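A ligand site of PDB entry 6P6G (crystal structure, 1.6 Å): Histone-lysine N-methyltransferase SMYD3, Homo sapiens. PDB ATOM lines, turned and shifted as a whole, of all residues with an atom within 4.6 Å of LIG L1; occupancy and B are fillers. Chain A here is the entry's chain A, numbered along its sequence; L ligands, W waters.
The side-chain carboxylate (OD2) of Asp 245 is in salt-bridge range of a nitrogen (N1) of LIG L1. The side-chain sulfur of Cys 184 sits at hydrogen-bond distance from an oxygen (O4) of LG2 L2, at 3.3 Å. The side-chain amide oxygen (OD1) of Asn 185 sits close to a sulfur (S1) of LG2 L2 (3.6 Å). O of Tyr 261 lies within hydrogen-bond range of O4 of LG2 L2 (2.6 Å). The backbone NH (N) of Thr 188 sits at hydrogen-bond distance from an oxygen (O3) of LIG L1. The backbone carbonyl oxygen (O) of Tyr 243 is in hydrogen-bond range of a nitrogen (N3) of LIG L1.
The side-chain amino group of Lys 333 is in salt-bridge range of the side-chain carboxylate of Asp 245 (3.7 Å). O of Lys 333 lies within hydrogen-bond range of SG of Cys 337 (3.3 Å). The backbone carbonyl oxygen of Thr 188 sits at hydrogen-bond distance from the side-chain sulfur of Cys 190 (3.6 Å). A ring nitrogen (ND1) of His 370 sits at hydrogen-bond distance from the backbone NH (N) of Val 372. The side-chain hydroxyl (OH) of Tyr 243 is in hydrogen-bond range of the backbone carbonyl oxygen (O) of Leu 208, 2.6 Å away. ND2 of Asn 185 sits close to SG of Cys 184.
F2 of LIG L1 sits close to OE1 of Glu 298 (3.5 Å). A fluorine (F1) of LIG L1 lies close to the side-chain sulfur (SG) of Cys 337, 3.7 Å away. Residues that only touch LIG L1: Glu 196 (3.1 Å), Leu 294 (3.3 Å), Tyr 261 (3.3 Å), Ser 186 (3.3 Å), Ile 241 (3.5 Å), Phe 187 (3.5 Å), Lys 333 (3.5 Å), Cys 190 (3.6 Å), Val 372 (3.6 Å), Cys 184 (3.6 Å), Met 194 (3.7 Å) and His 370 (3.9 Å). Hydrophobic or aromatic side chains that line LIG L1: Phe 187, Met 194, Ile 241, Tyr 243, Tyr 261, Leu 294, His 370 and Val 372. Of the 25 residues printed, 17 come within 4 Å of LIG L1. Along chain A the residues within 4 Å of LIG L1 span positions 184 to 372. The nearest printed residue that does not touch LIG L1 is Leu 244 (4.02 Å).
Water W2 bridges O of Ile 218 (2.8 Å) and O1 of LIG L1 (2.9 Å). Water W6 lies within hydrogen-bond range of NZ of Lys 301 and N1 of LIG L1. Water W4 lies within hydrogen-bond range of the backbone carbonyl oxygen (O) of Ser 186, the side-chain hydroxyl (OG1) of Thr 188 and an oxygen (O3) of LIG L1. Water W1 bridges O of Met 194 (2.7 Å) and NZ of Lys 301 (3.0 Å). Water W3 bridges the side-chain carboxylate of Asp 245 (2.6 Å) and the side-chain amino group of Lys 333 (2.9 Å).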
ATOM      1  N   CYS A 184      19.598  -5.627  -3.013  1.00  0.00           N
ATOM      2  CA  CYS A 184      18.845  -5.753  -4.246  1.00  0.00           C
ATOM      3  C   CYS A 184      18.504  -4.411  -4.885  1.00  0.00           C
ATOM      4  O   CYS A 184      18.006  -4.372  -6.014  1.00  0.00           O
ATOM      5  CB  CYS A 184      17.600  -6.563  -3.924  1.00  0.00           C
ATOM      6  SG  CYS A 184      16.243  -6.329  -5.008  1.00  0.00           S
ATOM      7  N   ASN A 185      18.717  -3.293  -4.181  1.00  0.00           N
ATOM      8  CA  ASN A 185      18.270  -2.009  -4.722  1.00  0.00           C
ATOM      9  C   ASN A 185      19.353  -0.929  -4.772  1.00  0.00           C
ATOM     10  O   ASN A 185      19.034   0.217  -5.071  1.00  0.00           O
ATOM     11  CB  ASN A 185      17.072  -1.490  -3.908  1.00  0.00           C
ATOM     12  CG  ASN A 185      15.837  -2.341  -4.118  1.00  0.00           C
ATOM     13  OD1 ASN A 185      15.179  -2.242  -5.152  1.00  0.00           O
ATOM     14  ND2 ASN A 185      15.557  -3.215  -3.171  1.00  0.00           N
ATOM     15  N   SER A 186      20.613  -1.279  -4.512  1.00  0.00           N
ATOM     16  CA  SER A 186      21.694  -0.302  -4.602  1.00  0.00           C
ATOM     17  C   SER A 186      22.031   0.010  -6.050  1.00  0.00           C
ATOM     18  O   SER A 186      22.141  -0.893  -6.881  1.00  0.00           O
ATOM     19  CB  SER A 186      22.938  -0.817  -3.888  1.00  0.00           C
ATOM     20  OG  SER A 186      22.785  -0.756  -2.484  1.00  0.00           O
ATOM     21  N   PHE A 187      22.242   1.296  -6.331  1.00  0.00           N
ATOM     22  CA  PHE A 187      22.709   1.754  -7.632  1.00  0.00           C
ATOM     23  C   PHE A 187      24.183   2.122  -7.560  1.00  0.00           C
ATOM     24  O   PHE A 187      24.625   2.803  -6.618  1.00  0.00           O
ATOM     25  CB  PHE A 187      21.920   2.978  -8.096  1.00  0.00           C
ATOM     26  CG  PHE A 187      20.527   2.682  -8.548  1.00  0.00           C
ATOM     27  CD1 PHE A 187      19.487   2.564  -7.629  1.00  0.00           C
ATOM     28  CD2 PHE A 187      20.242   2.547  -9.896  1.00  0.00           C
ATOM     29  CE1 PHE A 187      18.191   2.311  -8.051  1.00  0.00           C
ATOM     30  CE2 PHE A 187      18.943   2.279 -10.333  1.00  0.00           C
ATOM     31  CZ  PHE A 187      17.920   2.163  -9.414  1.00  0.00           C
ATOM     32  N   THR A 188      24.942   1.682  -8.561  1.00  0.00           N
ATOM     33  CA  THR A 188      26.348   2.042  -8.673  1.00  0.00           C
ATOM     34  C   THR A 188      26.444   3.384  -9.412  1.00  0.00           C
ATOM     35  O   THR A 188      26.152   3.455 -10.604  1.00  0.00           O
ATOM     36  CB  THR A 188      27.120   0.950  -9.407  1.00  0.00           C
ATOM     37  OG1 THR A 188      27.024  -0.277  -8.650  1.00  0.00           O
ATOM     38  CG2 THR A 188      28.575   1.334  -9.568  1.00  0.00           C
ATOM     39  N   CYS A 190      28.175   6.332 -11.260  1.00  0.00           N
ATOM     40  CA  CYS A 190      29.344   6.425 -12.137  1.00  0.00           C
ATOM     41  C   CYS A 190      29.623   7.874 -12.505  1.00  0.00           C
ATOM     42  O   CYS A 190      28.693   8.660 -12.701  1.00  0.00           O
ATOM     43  CB  CYS A 190      29.134   5.594 -13.411  1.00  0.00           C
ATOM     44  SG  CYS A 190      28.829   3.839 -13.040  1.00  0.00           S
ATOM     45  N   MET A 194      32.482   7.218 -16.640  1.00  0.00           N
ATOM     46  CA  MET A 194      31.963   5.882 -16.367  1.00  0.00           C
ATOM     47  C   MET A 194      32.818   5.103 -15.378  1.00  0.00           C
ATOM     48  O   MET A 194      32.749   3.874 -15.329  1.00  0.00           O
ATOM     49  CB  MET A 194      31.744   5.100 -17.668  1.00  0.00           C
ATOM     50  CG  MET A 194      30.584   5.664 -18.472  1.00  0.00           C
ATOM     51  SD  MET A 194      29.015   5.452 -17.590  1.00  0.00           S
ATOM     52  CE  MET A 194      27.876   6.184 -18.771  1.00  0.00           C
ATOM     53  N   GLU A 196      33.211   3.932 -11.642  1.00  0.00           N
ATOM     54  CA  GLU A 196      32.376   3.787 -10.456  1.00  0.00           C
ATOM     55  C   GLU A 196      32.936   4.631  -9.317  1.00  0.00           C
ATOM     56  O   GLU A 196      34.116   4.529  -8.978  1.00  0.00           O
ATOM     57  CB  GLU A 196      32.325   2.315 -10.033  1.00  0.00           C
ATOM     58  CG  GLU A 196      31.886   1.365 -11.141  1.00  0.00           C
ATOM     59  CD  GLU A 196      31.798  -0.074 -10.660  1.00  0.00           C
ATOM     60  OE1 GLU A 196      32.093  -0.332  -9.468  1.00  0.00           O
ATOM     61  OE2 GLU A 196      31.426  -0.950 -11.475  1.00  0.00           O
ATOM     62  N   SER A 206      13.945   2.512  -8.385  1.00  0.00           N
ATOM     63  CA  SER A 206      13.940   1.080  -8.117  1.00  0.00           C
ATOM     64  C   SER A 206      12.704   0.386  -8.654  1.00  0.00           C
ATOM     65  O   SER A 206      12.667  -0.852  -8.619  1.00  0.00           O
ATOM     66  CB  SER A 206      14.064   0.789  -6.620  1.00  0.00           C
ATOM     67  OG  SER A 206      15.409   0.860  -6.204  1.00  0.00           O
ATOM     68  N   LEU A 208      11.994   0.171 -11.694  1.00  0.00           N
ATOM     69  CA  LEU A 208      12.328  -0.343 -13.022  1.00  0.00           C
ATOM     70  C   LEU A 208      12.807  -1.779 -12.926  1.00  0.00           C
ATOM     71  O   LEU A 208      13.797  -2.082 -12.239  1.00  0.00           O
ATOM     72  CB  LEU A 208      13.404   0.519 -13.668  1.00  0.00           C
ATOM     73  CG  LEU A 208      12.985   1.929 -14.091  1.00  0.00           C
ATOM     74  CD1 LEU A 208      14.202   2.844 -14.134  1.00  0.00           C
ATOM     75  CD2 LEU A 208      12.314   1.866 -15.450  1.00  0.00           C
ATOM     76  N   ILE A 218      19.610   4.738 -17.537  1.00  0.00           N
ATOM     77  CA  ILE A 218      19.921   5.745 -16.519  1.00  0.00           C
ATOM     78  C   ILE A 218      21.363   6.190 -16.699  1.00  0.00           C
ATOM     79  O   ILE A 218      22.218   5.438 -17.181  1.00  0.00           O
ATOM     80  CB  ILE A 218      19.688   5.238 -15.078  1.00  0.00           C
ATOM     81  CG1 ILE A 218      20.606   4.042 -14.791  1.00  0.00           C
ATOM     82  CG2 ILE A 218      18.214   4.947 -14.843  1.00  0.00           C
ATOM     83  CD1 ILE A 218      20.640   3.613 -13.320  1.00  0.00           C
ATOM     84  N   PHE A 220      24.297   9.024 -14.606  1.00  0.00           N
ATOM     85  CA  PHE A 220      24.569   9.837 -13.432  1.00  0.00           C
ATOM     86  C   PHE A 220      25.309  11.106 -13.822  1.00  0.00           C
ATOM     87  O   PHE A 220      26.196  11.075 -14.689  1.00  0.00           O
ATOM     88  CB  PHE A 220      25.378   9.051 -12.394  1.00  0.00           C
ATOM     89  CG  PHE A 220      24.646   7.859 -11.867  1.00  0.00           C
ATOM     90  CD1 PHE A 220      23.766   7.992 -10.799  1.00  0.00           C
ATOM     91  CD2 PHE A 220      24.800   6.615 -12.470  1.00  0.00           C
ATOM     92  CE1 PHE A 220      23.067   6.896 -10.318  1.00  0.00           C
ATOM     93  CE2 PHE A 220      24.099   5.501 -11.991  1.00  0.00           C
ATOM     94  CZ  PHE A 220      23.229   5.645 -10.908  1.00  0.00           C
ATOM     95  N   ILE A 241      15.346  -1.166 -17.525  1.00  0.00           N
ATOM     96  CA  ILE A 241      16.755  -0.816 -17.701  1.00  0.00           C
ATOM     97  C   ILE A 241      17.540  -2.103 -17.593  1.00  0.00           C
ATOM     98  O   ILE A 241      17.028  -3.132 -17.132  1.00  0.00           O
ATOM     99  CB  ILE A 241      17.259   0.221 -16.669  1.00  0.00           C
ATOM    100  CG1 ILE A 241      17.031  -0.281 -15.235  1.00  0.00           C
ATOM    101  CG2 ILE A 241      16.598   1.570 -16.903  1.00  0.00           C
ATOM    102  CD1 ILE A 241      17.679   0.600 -14.166  1.00  0.00           C
ATOM    103  N   CYS A 242      18.795  -2.066 -18.034  1.00  0.00           N
ATOM    104  CA  CYS A 242      19.703  -3.181 -17.836  1.00  0.00           C
ATOM    105  C   CYS A 242      20.471  -2.954 -16.542  1.00  0.00           C
ATOM    106  O   CYS A 242      21.193  -1.958 -16.418  1.00  0.00           O
ATOM    107  CB  CYS A 242      20.648  -3.372 -19.020  1.00  0.00           C
ATOM    108  SG  CYS A 242      21.627  -4.890 -18.913  1.00  0.00           S
ATOM    109  N   TYR A 243      20.315  -3.858 -15.576  1.00  0.00           N
ATOM    110  CA  TYR A 243      21.010  -3.738 -14.300  1.00  0.00           C
ATOM    111  C   TYR A 243      22.506  -3.938 -14.425  1.00  0.00           C
ATOM    112  O   TYR A 243      23.234  -3.624 -13.482  1.00  0.00           O
ATOM    113  CB  TYR A 243      20.460  -4.769 -13.302  1.00  0.00           C
ATOM    114  CG  TYR A 243      19.016  -4.628 -12.854  1.00  0.00           C
ATOM    115  CD1 TYR A 243      18.240  -3.554 -13.252  1.00  0.00           C
ATOM    116  CD2 TYR A 243      18.445  -5.574 -12.008  1.00  0.00           C
ATOM    117  CE1 TYR A 243      16.922  -3.423 -12.840  1.00  0.00           C
ATOM    118  CE2 TYR A 243      17.124  -5.462 -11.568  1.00  0.00           C
ATOM    119  CZ  TYR A 243      16.375  -4.373 -11.995  1.00  0.00           C
ATOM    120  OH  TYR A 243      15.069  -4.244 -11.576  1.00  0.00           O
ATOM    121  N   LEU A 244      22.983  -4.468 -15.549  1.00  0.00           N
ATOM    122  CA  LEU A 244      24.307  -5.072 -15.645  1.00  0.00           C
ATOM    123  C   LEU A 244      25.172  -4.432 -16.729  1.00  0.00           C
ATOM    124  O   LEU A 244      24.674  -3.873 -17.713  1.00  0.00           O
ATOM    125  CB  LEU A 244      24.189  -6.573 -15.959  1.00  0.00           C
ATOM    126  CG  LEU A 244      23.305  -7.373 -15.015  1.00  0.00           C
ATOM    127  CD1 LEU A 244      23.249  -8.801 -15.518  1.00  0.00           C
ATOM    128  CD2 LEU A 244      23.942  -7.289 -13.648  1.00  0.00           C
ATOM    129  N   ASP A 245      26.482  -4.536 -16.531  1.00  0.00           N
ATOM    130  CA  ASP A 245      27.485  -4.321 -17.574  1.00  0.00           C
ATOM    131  C   ASP A 245      27.094  -5.097 -18.831  1.00  0.00           C
ATOM    132  O   ASP A 245      26.787  -6.288 -18.745  1.00  0.00           O
ATOM    133  CB  ASP A 245      28.836  -4.803 -17.036  1.00  0.00           C
ATOM    134  CG  ASP A 245      30.038  -4.383 -17.896  1.00  0.00           C
ATOM    135  OD1 ASP A 245      29.904  -4.245 -19.129  1.00  0.00           O
ATOM    136  OD2 ASP A 245      31.129  -4.224 -17.313  1.00  0.00           O
ATOM    137  N   TYR A 261      19.933 -10.393  -7.271  1.00  0.00           N
ATOM    138  CA  TYR A 261      18.557  -9.963  -7.506  1.00  0.00           C
ATOM    139  C   TYR A 261      17.542 -11.091  -7.387  1.00  0.00           C
ATOM    140  O   TYR A 261      16.341 -10.829  -7.516  1.00  0.00           O
ATOM    141  CB  TYR A 261      18.443  -9.316  -8.891  1.00  0.00           C
ATOM    142  CG  TYR A 261      19.278  -8.059  -9.005  1.00  0.00           C
ATOM    143  CD1 TYR A 261      18.859  -6.877  -8.418  1.00  0.00           C
ATOM    144  CD2 TYR A 261      20.484  -8.064  -9.703  1.00  0.00           C
ATOM    145  CE1 TYR A 261      19.603  -5.717  -8.528  1.00  0.00           C
ATOM    146  CE2 TYR A 261      21.259  -6.886  -9.805  1.00  0.00           C
ATOM    147  CZ  TYR A 261      20.791  -5.727  -9.211  1.00  0.00           C
ATOM    148  OH  TYR A 261      21.535  -4.568  -9.307  1.00  0.00           O
ATOM    149  N   LEU A 294      42.009  -9.880 -14.793  1.00  0.00           N
ATOM    150  CA  LEU A 294      41.121  -8.725 -14.714  1.00  0.00           C
ATOM    151  C   LEU A 294      40.553  -8.507 -13.318  1.00  0.00           C
ATOM    152  O   LEU A 294      40.114  -7.394 -13.016  1.00  0.00           O
ATOM    153  CB  LEU A 294      39.961  -8.884 -15.692  1.00  0.00           C
ATOM    154  CG  LEU A 294      40.199  -8.372 -17.126  1.00  0.00           C
ATOM    155  CD1 LEU A 294      39.079  -8.901 -18.018  1.00  0.00           C
ATOM    156  CD2 LEU A 294      40.227  -6.851 -17.179  1.00  0.00           C
ATOM    157  N   GLU A 298      40.694  -4.776 -12.303  1.00  0.00           N
ATOM    158  CA  GLU A 298      39.491  -4.054 -11.913  1.00  0.00           C
ATOM    159  C   GLU A 298      39.638  -3.440 -10.520  1.00  0.00           C
ATOM    160  O   GLU A 298      39.182  -2.328 -10.288  1.00  0.00           O
ATOM    161  CB  GLU A 298      38.286  -4.997 -11.957  1.00  0.00           C
ATOM    162  CG  GLU A 298      36.970  -4.354 -11.534  1.00  0.00           C
ATOM    163  CD  GLU A 298      35.792  -5.313 -11.571  1.00  0.00           C
ATOM    164  OE1 GLU A 298      36.017  -6.539 -11.445  1.00  0.00           O
ATOM    165  OE2 GLU A 298      34.649  -4.843 -11.728  1.00  0.00           O
ATOM    166  N   LYS A 301      41.917  -0.406 -10.873  1.00  0.00           N
ATOM    167  CA  LYS A 301      41.191   0.686 -11.498  1.00  0.00           C
ATOM    168  C   LYS A 301      40.209   1.327 -10.524  1.00  0.00           C
ATOM    169  O   LYS A 301      40.077   2.558 -10.481  1.00  0.00           O
ATOM    170  CB  LYS A 301      40.463   0.178 -12.737  1.00  0.00           C
ATOM    171  CG  LYS A 301      39.572   1.214 -13.420  1.00  0.00           C
ATOM    172  CD  LYS A 301      39.001   0.686 -14.724  1.00  0.00           C
ATOM    173  CE  LYS A 301      38.243   1.764 -15.470  1.00  0.00           C
ATOM    174  NZ  LYS A 301      36.935   2.042 -14.833  1.00  0.00           N
ATOM    175  N   LYS A 333      37.891  -5.548 -22.255  1.00  0.00           N
ATOM    176  CA  LYS A 333      37.980  -4.905 -20.953  1.00  0.00           C
ATOM    177  C   LYS A 333      39.397  -4.432 -20.679  1.00  0.00           C
ATOM    178  O   LYS A 333      39.599  -3.348 -20.096  1.00  0.00           O
ATOM    179  CB  LYS A 333      37.494  -5.872 -19.874  1.00  0.00           C
ATOM    180  CG  LYS A 333      35.993  -6.137 -19.928  1.00  0.00           C
ATOM    181  CD  LYS A 333      35.640  -7.348 -19.050  1.00  0.00           C
ATOM    182  CE  LYS A 333      34.211  -7.823 -19.246  1.00  0.00           C
ATOM    183  NZ  LYS A 333      33.225  -6.956 -18.547  1.00  0.00           N
ATOM    184  N   CYS A 337      40.473  -0.542 -19.944  1.00  0.00           N
ATOM    185  CA  CYS A 337      41.218  -0.116 -18.771  1.00  0.00           C
ATOM    186  C   CYS A 337      42.531   0.536 -19.170  1.00  0.00           C
ATOM    187  O   CYS A 337      42.942   1.548 -18.584  1.00  0.00           O
ATOM    188  CB  CYS A 337      41.467  -1.303 -17.844  1.00  0.00           C
ATOM    189  SG  CYS A 337      39.959  -2.015 -17.093  1.00  0.00           S
ATOM    190  N   HIS A 370      23.383   3.586 -26.044  1.00  0.00           N
ATOM    191  CA  HIS A 370      23.812   3.187 -24.708  1.00  0.00           C
ATOM    192  C   HIS A 370      24.798   4.245 -24.207  1.00  0.00           C
ATOM    193  O   HIS A 370      25.748   4.597 -24.919  1.00  0.00           O
ATOM    194  CB  HIS A 370      24.471   1.800 -24.709  1.00  0.00           C
ATOM    195  CG  HIS A 370      24.669   1.228 -23.336  1.00  0.00           C
ATOM    196  ND1 HIS A 370      25.569   1.741 -22.436  1.00  0.00           N
ATOM    197  CD2 HIS A 370      24.114   0.148 -22.742  1.00  0.00           C
ATOM    198  CE1 HIS A 370      25.546   1.018 -21.322  1.00  0.00           C
ATOM    199  NE2 HIS A 370      24.666   0.044 -21.481  1.00  0.00           N
ATOM    200  N   VAL A 372      27.311   4.155 -22.229  1.00  0.00           N
ATOM    201  CA  VAL A 372      28.707   3.751 -22.121  1.00  0.00           C
ATOM    202  C   VAL A 372      29.391   3.830 -23.493  1.00  0.00           C
ATOM    203  O   VAL A 372      30.550   4.248 -23.588  1.00  0.00           O
ATOM    204  CB  VAL A 372      28.819   2.343 -21.505  1.00  0.00           C
ATOM    205  CG1 VAL A 372      30.204   1.765 -21.742  1.00  0.00           C
ATOM    206  CG2 VAL A 372      28.511   2.410 -20.002  1.00  0.00           C
HETATM  207  C1  LIG L   1      31.281  -0.768 -16.810  1.00  0.00           C
HETATM  208  C2  LIG L   1      28.445   1.821 -16.378  1.00  0.00           C
HETATM  209  C3  LIG L   1      24.641  -0.285 -13.221  1.00  0.00           C
HETATM  210  C4  LIG L   1      24.858  -1.070 -14.495  1.00  0.00           C
HETATM  211  C5  LIG L   1      26.188  -0.699 -15.115  1.00  0.00           C
HETATM  212  C6  LIG L   1      22.936  -0.368 -11.464  1.00  0.00           C
HETATM  213  C7  LIG L   1      21.509  -0.684 -11.202  1.00  0.00           C
HETATM  214  C8  LIG L   1      19.647  -1.282 -10.276  1.00  0.00           C
HETATM  215  C9  LIG L   1      36.825  -4.486 -15.550  1.00  0.00           C
HETATM  216  C10 LIG L   1      35.687  -3.802 -16.202  1.00  0.00           C
HETATM  217  C11 LIG L   1      34.920  -2.915 -15.263  1.00  0.00           C
HETATM  218  C12 LIG L   1      34.008  -1.973 -16.019  1.00  0.00           C
HETATM  219  C13 LIG L   1      32.142  -0.394 -15.625  1.00  0.00           C
HETATM  220  C14 LIG L   1      30.277   0.324 -17.165  1.00  0.00           C
HETATM  221  C15 LIG L   1      29.388   0.677 -15.990  1.00  0.00           C
HETATM  222  C16 LIG L   1      26.101   1.537 -14.138  1.00  0.00           C
HETATM  223  C17 LIG L   1      24.784   1.220 -13.452  1.00  0.00           C
HETATM  224  C18 LIG L   1      20.938  -1.117  -9.998  1.00  0.00           C
HETATM  225  C19 LIG L   1      18.646  -1.742  -9.263  1.00  0.00           C
HETATM  226  C20 LIG L   1      30.276   1.125 -14.831  1.00  0.00           C
HETATM  227  C21 LIG L   1      31.299   0.051 -14.447  1.00  0.00           C
HETATM  228  F1  LIG L   1      37.597  -3.663 -14.844  1.00  0.00           F
HETATM  229  F2  LIG L   1      36.471  -5.433 -14.726  1.00  0.00           F
HETATM  230  F3  LIG L   1      37.603  -5.055 -16.450  1.00  0.00           F
HETATM  231  N1  LIG L   1      32.821  -1.630 -15.218  1.00  0.00           N
HETATM  232  N2  LIG L   1      26.186   0.739 -15.369  1.00  0.00           N
HETATM  233  N3  LIG L   1      23.299  -0.561 -12.739  1.00  0.00           N
HETATM  234  N4  LIG L   1      20.618  -0.600 -12.180  1.00  0.00           N
HETATM  235  O1  LIG L   1      26.031   2.495 -17.090  1.00  0.00           O
HETATM  236  O2  LIG L   1      26.822   0.234 -17.696  1.00  0.00           O
HETATM  237  O3  LIG L   1      23.700   0.031 -10.589  1.00  0.00           O
HETATM  238  O4  LIG L   1      19.386  -0.984 -11.574  1.00  0.00           O
HETATM  239  S1  LIG L   1      26.785   1.327 -16.766  1.00  0.00           S
HETATM  240  C22 LIG L   1      17.895  -3.033  -9.363  1.00  0.00           C
HETATM  241  C23 LIG L   1      17.173  -1.762  -9.599  1.00  0.00           C
HETATM  242  N1  LG2 L   2       9.989  -5.622  -9.104  1.00  0.00           N
HETATM  243  C1  LG2 L   2      10.651  -4.751  -8.120  1.00  0.00           C
HETATM  244  C2  LG2 L   2      11.223  -3.519  -8.800  1.00  0.00           C
HETATM  245  C3  LG2 L   2      12.633  -3.780  -9.351  1.00  0.00           C
HETATM  246  S1  LG2 L   2      13.799  -4.009  -7.976  1.00  0.00           S
HETATM  247  C4  LG2 L   2       9.696  -4.394  -6.986  1.00  0.00           C
HETATM  248  O1  LG2 L   2      10.001  -3.562  -6.138  1.00  0.00           O
HETATM  249  O2  LG2 L   2       8.596  -4.953  -6.904  1.00  0.00           O
HETATM  250  C5  LG2 L   2      14.587  -5.560  -8.521  1.00  0.00           C
HETATM  251  C6  LG2 L   2      13.788  -6.828  -8.231  1.00  0.00           C
HETATM  252  O3  LG2 L   2      12.716  -6.897  -9.135  1.00  0.00           O
HETATM  253  C7  LG2 L   2      14.584  -8.105  -8.469  1.00  0.00           C
HETATM  254  O4  LG2 L   2      15.316  -8.481  -7.310  1.00  0.00           O
HETATM  255  C8  LG2 L   2      13.507  -9.090  -8.833  1.00  0.00           C
HETATM  256  O5  LG2 L   2      12.791  -9.444  -7.668  1.00  0.00           O
HETATM  257  C9  LG2 L   2      12.585  -8.215  -9.634  1.00  0.00           C
HETATM  258  N2  LG2 L   2      12.925  -8.178 -11.077  1.00  0.00           N
HETATM  259  C10 LG2 L   2      13.565  -7.165 -11.751  1.00  0.00           C
HETATM  260  N3  LG2 L   2      13.663  -7.507 -13.065  1.00  0.00           N
HETATM  261  C11 LG2 L   2      13.081  -8.732 -13.213  1.00  0.00           C
HETATM  262  C12 LG2 L   2      12.904  -9.580 -14.303  1.00  0.00           C
HETATM  263  N4  LG2 L   2      13.307  -9.250 -15.531  1.00  0.00           N
HETATM  264  N5  LG2 L   2      12.282 -10.789 -14.103  1.00  0.00           N
HETATM  265  C13 LG2 L   2      11.830 -11.170 -12.863  1.00  0.00           C
HETATM  266  N6  LG2 L   2      12.008 -10.352 -11.780  1.00  0.00           N
HETATM  267  C14 LG2 L   2      12.627  -9.161 -11.967  1.00  0.00           C
HETATM  268  O   HOH W   1      34.427   2.067 -16.480  1.00  0.00           O
HETATM  269  O   HOH W   2      25.017   5.173 -17.184  1.00  0.00           O
HETATM  270  O   HOH W   3      33.339  -4.112 -18.767  1.00  0.00           O
HETATM  271  O   HOH W   4      24.429  -2.302  -8.338  1.00  0.00           O
HETATM  272  O   HOH W   5      30.326  -1.662 -19.973  1.00  0.00           O
HETATM  273  O   HOH W   6      35.512  -0.201 -13.683  1.00  0.00           O
HETATM  274  O   HOH W   7      27.561  -1.511 -19.846  1.00  0.00           O
